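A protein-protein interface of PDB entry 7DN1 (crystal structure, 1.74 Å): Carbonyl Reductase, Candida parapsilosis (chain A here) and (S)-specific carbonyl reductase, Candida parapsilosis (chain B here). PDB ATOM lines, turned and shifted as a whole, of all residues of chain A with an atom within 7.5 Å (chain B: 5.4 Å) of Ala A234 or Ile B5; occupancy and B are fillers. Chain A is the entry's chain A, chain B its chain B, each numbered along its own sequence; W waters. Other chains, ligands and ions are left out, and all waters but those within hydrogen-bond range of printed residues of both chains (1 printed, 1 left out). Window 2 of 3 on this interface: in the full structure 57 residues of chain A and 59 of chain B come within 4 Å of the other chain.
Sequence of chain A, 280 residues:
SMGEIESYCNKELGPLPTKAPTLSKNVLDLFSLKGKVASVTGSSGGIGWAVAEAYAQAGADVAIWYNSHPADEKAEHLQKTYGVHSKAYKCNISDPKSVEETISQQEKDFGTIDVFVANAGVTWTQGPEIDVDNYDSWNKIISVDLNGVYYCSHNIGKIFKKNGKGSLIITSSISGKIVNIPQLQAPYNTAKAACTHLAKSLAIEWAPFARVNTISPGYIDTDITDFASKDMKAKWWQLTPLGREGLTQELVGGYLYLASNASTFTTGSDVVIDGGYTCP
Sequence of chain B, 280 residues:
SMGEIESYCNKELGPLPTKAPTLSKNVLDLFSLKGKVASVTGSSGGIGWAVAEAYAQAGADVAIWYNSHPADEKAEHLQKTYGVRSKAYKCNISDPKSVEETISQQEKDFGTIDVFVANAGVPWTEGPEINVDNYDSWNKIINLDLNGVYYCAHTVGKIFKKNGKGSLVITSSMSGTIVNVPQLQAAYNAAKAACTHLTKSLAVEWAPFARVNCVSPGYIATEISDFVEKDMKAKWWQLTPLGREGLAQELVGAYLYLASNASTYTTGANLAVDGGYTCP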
ATOM      1  N   SER A 229      34.998   2.328   4.015  1.00  0.00           N
ATOM      2  CA  SER A 229      33.774   2.415   4.795  1.00  0.00           C
ATOM      3  C   SER A 229      32.807   1.301   4.396  1.00  0.00           C
ATOM      4  O   SER A 229      32.996   0.603   3.396  1.00  0.00           O
ATOM      5  CB  SER A 229      33.103   3.773   4.592  1.00  0.00           C
ATOM      6  OG  SER A 229      32.852   4.003   3.215  1.00  0.00           O
ATOM      7  N   LYS A 230      31.735   1.159   5.181  1.00  0.00           N
ATOM      8  CA  LYS A 230      30.755   0.109   4.910  1.00  0.00           C
ATOM      9  C   LYS A 230      30.061   0.319   3.572  1.00  0.00           C
ATOM     10  O   LYS A 230      29.810  -0.643   2.840  1.00  0.00           O
ATOM     11  CB  LYS A 230      29.719   0.043   6.033  1.00  0.00           C
ATOM     12  CG  LYS A 230      28.761  -1.147   5.925  1.00  0.00           C
ATOM     13  CD  LYS A 230      27.795  -1.156   7.115  1.00  0.00           C
ATOM     14  CE  LYS A 230      26.949  -2.427   7.187  1.00  0.00           C
ATOM     15  NZ  LYS A 230      26.091  -2.639   5.984  1.00  0.00           N
ATOM     16  N   ASP A 231      29.727   1.562   3.235  1.00  0.00           N
ATOM     17  CA  ASP A 231      29.043   1.772   1.967  1.00  0.00           C
ATOM     18  C   ASP A 231      29.958   1.496   0.778  1.00  0.00           C
ATOM     19  O   ASP A 231      29.466   1.183  -0.310  1.00  0.00           O
ATOM     20  CB  ASP A 231      28.477   3.188   1.886  1.00  0.00           C
ATOM     21  CG  ASP A 231      27.145   3.334   2.626  1.00  0.00           C
ATOM     22  OD1 ASP A 231      26.699   2.373   3.288  1.00  0.00           O
ATOM     23  OD2 ASP A 231      26.523   4.410   2.516  1.00  0.00           O
ATOM     24  N   MET A 232      31.275   1.577   0.955  1.00  0.00           N
ATOM     25  CA  MET A 232      32.128   1.255  -0.178  1.00  0.00           C
ATOM     26  C   MET A 232      32.272  -0.255  -0.318  1.00  0.00           C
ATOM     27  O   MET A 232      32.125  -0.779  -1.425  1.00  0.00           O
ATOM     28  CB  MET A 232      33.482   1.948  -0.044  1.00  0.00           C
ATOM     29  CG  MET A 232      34.630   1.290  -0.804  1.00  0.00           C
ATOM     30  SD  MET A 232      36.111   2.252  -0.457  1.00  0.00           S
ATOM     31  CE  MET A 232      35.579   3.844  -1.107  1.00  0.00           C
ATOM     32  N   LYS A 233      32.495  -0.973   0.798  1.00  0.00           N
ATOM     33  CA  LYS A 233      32.505  -2.439   0.740  1.00  0.00           C
ATOM     34  C   LYS A 233      31.209  -2.982   0.161  1.00  0.00           C
ATOM     35  O   LYS A 233      31.215  -3.966  -0.581  1.00  0.00           O
ATOM     36  CB  LYS A 233      32.690  -3.066   2.123  1.00  0.00           C
ATOM     37  CG  LYS A 233      34.042  -3.007   2.794  1.00  0.00           C
ATOM     38  CD  LYS A 233      34.119  -4.272   3.670  1.00  0.00           C
ATOM     39  CE  LYS A 233      35.135  -4.217   4.791  1.00  0.00           C
ATOM     40  NZ  LYS A 233      34.456  -3.838   6.069  1.00  0.00           N
ATOM     41  N   ALA A 234      30.076  -2.386   0.539  1.00  0.00           N
ATOM     42  CA  ALA A 234      28.799  -2.875   0.038  1.00  0.00           C
ATOM     43  C   ALA A 234      28.750  -2.835  -1.480  1.00  0.00           C
ATOM     44  O   ALA A 234      28.225  -3.753  -2.118  1.00  0.00           O
ATOM     45  CB  ALA A 234      27.649  -2.067   0.639  1.00  0.00           C
ATOM     46  N   LYS A 235      29.311  -1.785  -2.085  1.00  0.00           N
ATOM     47  CA  LYS A 235      29.317  -1.726  -3.537  1.00  0.00           C
ATOM     48  C   LYS A 235      30.226  -2.790  -4.126  1.00  0.00           C
ATOM     49  O   LYS A 235      29.905  -3.355  -5.176  1.00  0.00           O
ATOM     50  CB  LYS A 235      29.704  -0.317  -3.996  1.00  0.00           C
ATOM     51  CG  LYS A 235      28.705   0.710  -3.497  1.00  0.00           C
ATOM     52  CD  LYS A 235      28.805   2.045  -4.219  1.00  0.00           C
ATOM     53  CE  LYS A 235      27.771   3.029  -3.654  1.00  0.00           C
ATOM     54  NZ  LYS A 235      27.998   3.310  -2.205  1.00  0.00           N
ATOM     55  N   TRP A 236      31.349  -3.093  -3.465  1.00  0.00           N
ATOM     56  CA  TRP A 236      32.171  -4.214  -3.911  1.00  0.00           C
ATOM     57  C   TRP A 236      31.361  -5.508  -3.932  1.00  0.00           C
ATOM     58  O   TRP A 236      31.395  -6.248  -4.918  1.00  0.00           O
ATOM     59  CB  TRP A 236      33.397  -4.387  -3.018  1.00  0.00           C
ATOM     60  CG  TRP A 236      34.336  -3.250  -2.926  1.00  0.00           C
ATOM     61  CD1 TRP A 236      34.411  -2.154  -3.739  1.00  0.00           C
ATOM     62  CD2 TRP A 236      35.382  -3.112  -1.964  1.00  0.00           C
ATOM     63  NE1 TRP A 236      35.429  -1.330  -3.315  1.00  0.00           N
ATOM     64  CE2 TRP A 236      36.043  -1.902  -2.233  1.00  0.00           C
ATOM     65  CE3 TRP A 236      35.833  -3.910  -0.907  1.00  0.00           C
ATOM     66  CZ2 TRP A 236      37.129  -1.463  -1.474  1.00  0.00           C
ATOM     67  CZ3 TRP A 236      36.901  -3.470  -0.152  1.00  0.00           C
ATOM     68  CH2 TRP A 236      37.539  -2.257  -0.440  1.00  0.00           C
ATOM     69  N   TRP A 237      30.617  -5.791  -2.851  1.00  0.00           N
ATOM     70  CA  TRP A 237      29.814  -7.016  -2.801  1.00  0.00           C
ATOM     71  C   TRP A 237      28.786  -7.048  -3.926  1.00  0.00           C
ATOM     72  O   TRP A 237      28.525  -8.111  -4.509  1.00  0.00           O
ATOM     73  CB  TRP A 237      29.096  -7.154  -1.457  1.00  0.00           C
ATOM     74  CG  TRP A 237      29.966  -7.093  -0.257  1.00  0.00           C
ATOM     75  CD1 TRP A 237      31.280  -7.425  -0.169  1.00  0.00           C
ATOM     76  CD2 TRP A 237      29.569  -6.662   1.050  1.00  0.00           C
ATOM     77  NE1 TRP A 237      31.730  -7.240   1.118  1.00  0.00           N
ATOM     78  CE2 TRP A 237      30.697  -6.777   1.887  1.00  0.00           C
ATOM     79  CE3 TRP A 237      28.374  -6.197   1.586  1.00  0.00           C
ATOM     80  CZ2 TRP A 237      30.669  -6.422   3.228  1.00  0.00           C
ATOM     81  CZ3 TRP A 237      28.339  -5.851   2.919  1.00  0.00           C
ATOM     82  CH2 TRP A 237      29.479  -5.979   3.732  1.00  0.00           C
ATOM     83  N   GLN A 238      28.171  -5.893  -4.224  1.00  0.00           N
ATOM     84  CA  GLN A 238      27.128  -5.828  -5.246  1.00  0.00           C
ATOM     85  C   GLN A 238      27.658  -6.163  -6.628  1.00  0.00           C
ATOM     86  O   GLN A 238      26.894  -6.622  -7.487  1.00  0.00           O
ATOM     87  CB  GLN A 238      26.502  -4.433  -5.271  1.00  0.00           C
ATOM     88  CG  GLN A 238      25.503  -4.173  -4.141  1.00  0.00           C
ATOM     89  CD  GLN A 238      24.937  -2.772  -4.213  1.00  0.00           C
ATOM     90  OE1 GLN A 238      25.685  -1.801  -4.387  1.00  0.00           O
ATOM     91  NE2 GLN A 238      23.621  -2.658  -4.123  1.00  0.00           N
ATOM     92  N   LEU A 239      28.943  -5.923  -6.863  1.00  0.00           N
ATOM     93  CA  LEU A 239      29.554  -6.099  -8.168  1.00  0.00           C
ATOM     94  C   LEU A 239      30.342  -7.400  -8.271  1.00  0.00           C
ATOM     95  O   LEU A 239      30.893  -7.691  -9.333  1.00  0.00           O
ATOM     96  CB  LEU A 239      30.452  -4.890  -8.464  1.00  0.00           C
ATOM     97  CG  LEU A 239      29.707  -3.645  -8.999  1.00  0.00           C
ATOM     98  CD1 LEU A 239      29.058  -3.983 -10.331  1.00  0.00           C
ATOM     99  CD2 LEU A 239      28.664  -3.140  -8.077  1.00  0.00           C
ATOM    100  N   THR A 240      30.381  -8.197  -7.198  1.00  0.00           N
ATOM    101  CA  THR A 240      31.093  -9.472  -7.168  1.00  0.00           C
ATOM    102  C   THR A 240      30.105 -10.600  -7.411  1.00  0.00           C
ATOM    103  O   THR A 240      29.199 -10.782  -6.584  1.00  0.00           O
ATOM    104  CB  THR A 240      31.763  -9.676  -5.811  1.00  0.00           C
ATOM    105  OG1 THR A 240      32.620  -8.563  -5.516  1.00  0.00           O
ATOM    106  CG2 THR A 240      32.594 -11.004  -5.806  1.00  0.00           C
ATOM    107  N   GLY A 243      29.196 -12.546  -4.432  1.00  0.00           N
ATOM    108  CA  GLY A 243      28.425 -11.770  -3.451  1.00  0.00           C
ATOM    109  C   GLY A 243      29.134 -11.453  -2.147  1.00  0.00           C
ATOM    110  O   GLY A 243      28.472 -11.056  -1.173  1.00  0.00           O
ATOM    111  N   GLU A 245      33.428 -10.813  -0.160  1.00  0.00           N
ATOM    112  CA  GLU A 245      34.881 -10.835  -0.221  1.00  0.00           C
ATOM    113  C   GLU A 245      35.379 -12.267  -0.005  1.00  0.00           C
ATOM    114  O   GLU A 245      34.689 -13.111   0.572  1.00  0.00           O
ATOM    115  CB  GLU A 245      35.480  -9.918   0.851  1.00  0.00           C
ATOM    116  CG  GLU A 245      35.236  -8.419   0.626  1.00  0.00           C
ATOM    117  CD  GLU A 245      35.450  -7.586   1.887  1.00  0.00           C
ATOM    118  OE1 GLU A 245      34.448  -7.102   2.453  1.00  0.00           O
ATOM    119  OE2 GLU A 245      36.608  -7.399   2.318  1.00  0.00           O
ATOM    120  N   GLY B   3      16.297  -2.351   3.216  1.00  0.00           N
ATOM    121  CA  GLY B   3      17.241  -2.781   4.215  1.00  0.00           C
ATOM    122  C   GLY B   3      18.195  -3.861   3.761  1.00  0.00           C
ATOM    123  O   GLY B   3      19.190  -4.108   4.442  1.00  0.00           O
ATOM    124  N   GLU B   4      17.909  -4.528   2.654  1.00  0.00           N
ATOM    125  CA  GLU B   4      18.831  -5.525   2.139  1.00  0.00           C
ATOM    126  C   GLU B   4      19.761  -4.866   1.142  1.00  0.00           C
ATOM    127  O   GLU B   4      19.374  -3.949   0.408  1.00  0.00           O
ATOM    128  CB  GLU B   4      18.081  -6.670   1.464  1.00  0.00           C
ATOM    129  CG  GLU B   4      16.985  -7.263   2.348  1.00  0.00           C
ATOM    130  CD  GLU B   4      16.002  -8.103   1.557  1.00  0.00           C
ATOM    131  OE1 GLU B   4      15.074  -8.662   2.182  1.00  0.00           O
ATOM    132  OE2 GLU B   4      16.174  -8.210   0.318  1.00  0.00           O
ATOM    133  N   ILE B   5      20.997  -5.331   1.122  1.00  0.00           N
ATOM    134  CA  ILE B   5      21.899  -5.008   0.024  1.00  0.00           C
ATOM    135  C   ILE B   5      21.647  -6.023  -1.078  1.00  0.00           C
ATOM    136  O   ILE B   5      21.935  -7.212  -0.909  1.00  0.00           O
ATOM    137  CB  ILE B   5      23.361  -5.034   0.474  1.00  0.00           C
ATOM    138  CG1 ILE B   5      23.615  -3.994   1.554  1.00  0.00           C
ATOM    139  CG2 ILE B   5      24.288  -4.794  -0.727  1.00  0.00           C
ATOM    140  CD1 ILE B   5      24.878  -4.237   2.362  1.00  0.00           C
ATOM    141  N   GLU B   6      21.126  -5.555  -2.214  1.00  0.00           N
ATOM    142  CA  GLU B   6      20.794  -6.432  -3.329  1.00  0.00           C
ATOM    143  C   GLU B   6      21.905  -6.413  -4.375  1.00  0.00           C
ATOM    144  O   GLU B   6      22.425  -5.352  -4.724  1.00  0.00           O
ATOM    145  CB  GLU B   6      19.468  -6.002  -3.958  1.00  0.00           C
ATOM    146  CG  GLU B   6      18.978  -6.883  -5.105  1.00  0.00           C
ATOM    147  CD  GLU B   6      17.806  -6.249  -5.855  1.00  0.00           C
ATOM    148  OE1 GLU B   6      18.013  -5.767  -6.994  1.00  0.00           O
ATOM    149  OE2 GLU B   6      16.686  -6.203  -5.289  1.00  0.00           O
ATOM    150  N   SER B   7      22.264  -7.596  -4.868  1.00  0.00           N
ATOM    151  CA  SER B   7      23.334  -7.712  -5.852  1.00  0.00           C
ATOM    152  C   SER B   7      22.962  -7.013  -7.153  1.00  0.00           C
ATOM    153  O   SER B   7      21.812  -7.072  -7.607  1.00  0.00           O
ATOM    154  CB  SER B   7      23.619  -9.193  -6.114  1.00  0.00           C
ATOM    155  OG  SER B   7      24.536  -9.360  -7.185  1.00  0.00           O
ATOM    156  N   GLY B  14      20.498 -13.406  -2.768  1.00  0.00           N
ATOM    157  CA  GLY B  14      19.901 -12.962  -1.524  1.00  0.00           C
ATOM    158  C   GLY B  14      20.591 -11.734  -0.961  1.00  0.00           C
ATOM    159  O   GLY B  14      21.479 -11.163  -1.600  1.00  0.00           O
ATOM    160  N   PRO B  15      20.192 -11.296   0.236  1.00  0.00           N
ATOM    161  CA  PRO B  15      20.816 -10.112   0.850  1.00  0.00           C
ATOM    162  C   PRO B  15      22.307 -10.315   1.061  1.00  0.00           C
ATOM    163  O   PRO B  15      22.744 -11.346   1.575  1.00  0.00           O
ATOM    164  CB  PRO B  15      20.076  -9.971   2.184  1.00  0.00           C
ATOM    165  CG  PRO B  15      18.809 -10.688   1.987  1.00  0.00           C
ATOM    166  CD  PRO B  15      19.120 -11.839   1.086  1.00  0.00           C
ATOM    167  N   LEU B  16      23.091  -9.317   0.660  1.00  0.00           N
ATOM    168  CA  LEU B  16      24.539  -9.446   0.699  1.00  0.00           C
ATOM    169  C   LEU B  16      25.073  -8.967   2.043  1.00  0.00           C
ATOM    170  O   LEU B  16      24.421  -8.189   2.734  1.00  0.00           O
ATOM    171  CB  LEU B  16      25.162  -8.642  -0.445  1.00  0.00           C
ATOM    172  CG  LEU B  16      24.688  -9.016  -1.836  1.00  0.00           C
ATOM    173  CD1 LEU B  16      25.462  -8.168  -2.864  1.00  0.00           C
ATOM    174  CD2 LEU B  16      24.932 -10.507  -2.116  1.00  0.00           C
ATOM    175  N   PRO B  17      26.267  -9.424   2.459  1.00  0.00           N
ATOM    176  CA  PRO B  17      27.107 -10.371   1.723  1.00  0.00           C
ATOM    177  C   PRO B  17      26.702 -11.821   1.925  1.00  0.00           C
ATOM    178  O   PRO B  17      26.136 -12.169   2.958  1.00  0.00           O
ATOM    179  CB  PRO B  17      28.503 -10.115   2.296  1.00  0.00           C
ATOM    180  CG  PRO B  17      28.272  -9.743   3.679  1.00  0.00           C
ATOM    181  CD  PRO B  17      26.910  -8.983   3.711  1.00  0.00           C
HETATM  182  O   HOH W   1      20.474  -2.665  -2.686  1.00  0.00           O
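Of the 9 printed residues of chain B, 5 touch a printed residue of chain A. Hydrophobic or aromatic side chains of chain B that line the printed part of chain A: Ile B5, Leu B16 and Pro B17. Among the printed residues, 10 pairs touch across the chains.
Of the printed residues of chain B, Ala A234 touches Ile B5. Trp A236 touches none of the printed residues of chain B. Of the printed residues of chain B, Gln A238 touches Ile B5 (3.7 Å), Glu B6 (3.0 Å), Ser B7 (3.6 Å) and Leu B16 (3.7 Å). Of the printed residues of chain B, Gly A243 touches Leu B16 and Pro B17. Ile B5 touches three residues of chain A. Pro B15 touches none of the printed residues of chain A. Printed residues of chain A within 4 Å of Pro B17: Trp A237 (3.5 Å) and Gly A243 (3.3 Å). The nearest residue of chain A that does not touch Ile B5 is Lys A230 (4.1 Å). The nearest printed residue of chain A that does not touch Pro B17 is Glu A245 (5.5 Å).
Water W1 lies within hydrogen-bond range of N of Glu B6 (3.0 Å) and NE2 of Gln A238 (3.5 Å).
The backbone carbonyl oxygen of Glu B6 is in hydrogen-bond range of the side-chain amide nitrogen of Gln A238, 3.0 Å away.
N of Leu B16 lies within hydrogen-bond range of O of Ile B5 (2.9 Å). NE1 of Trp A237 is in hydrogen-bond range of OE1 of Glu A245 (3.0 Å).
Among the printed residues, merely in contact across the chains: Gly A243 with Pro B17, Trp A237 with Leu B16, Trp A237 with Pro B17, Gln A238 with Ser B7, Gln A238 with Ile B5, Gly A243 with Leu B16, Gln A238 with Leu B16, Trp A237 with Ile B5 and Ala A234 with Ile B5.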
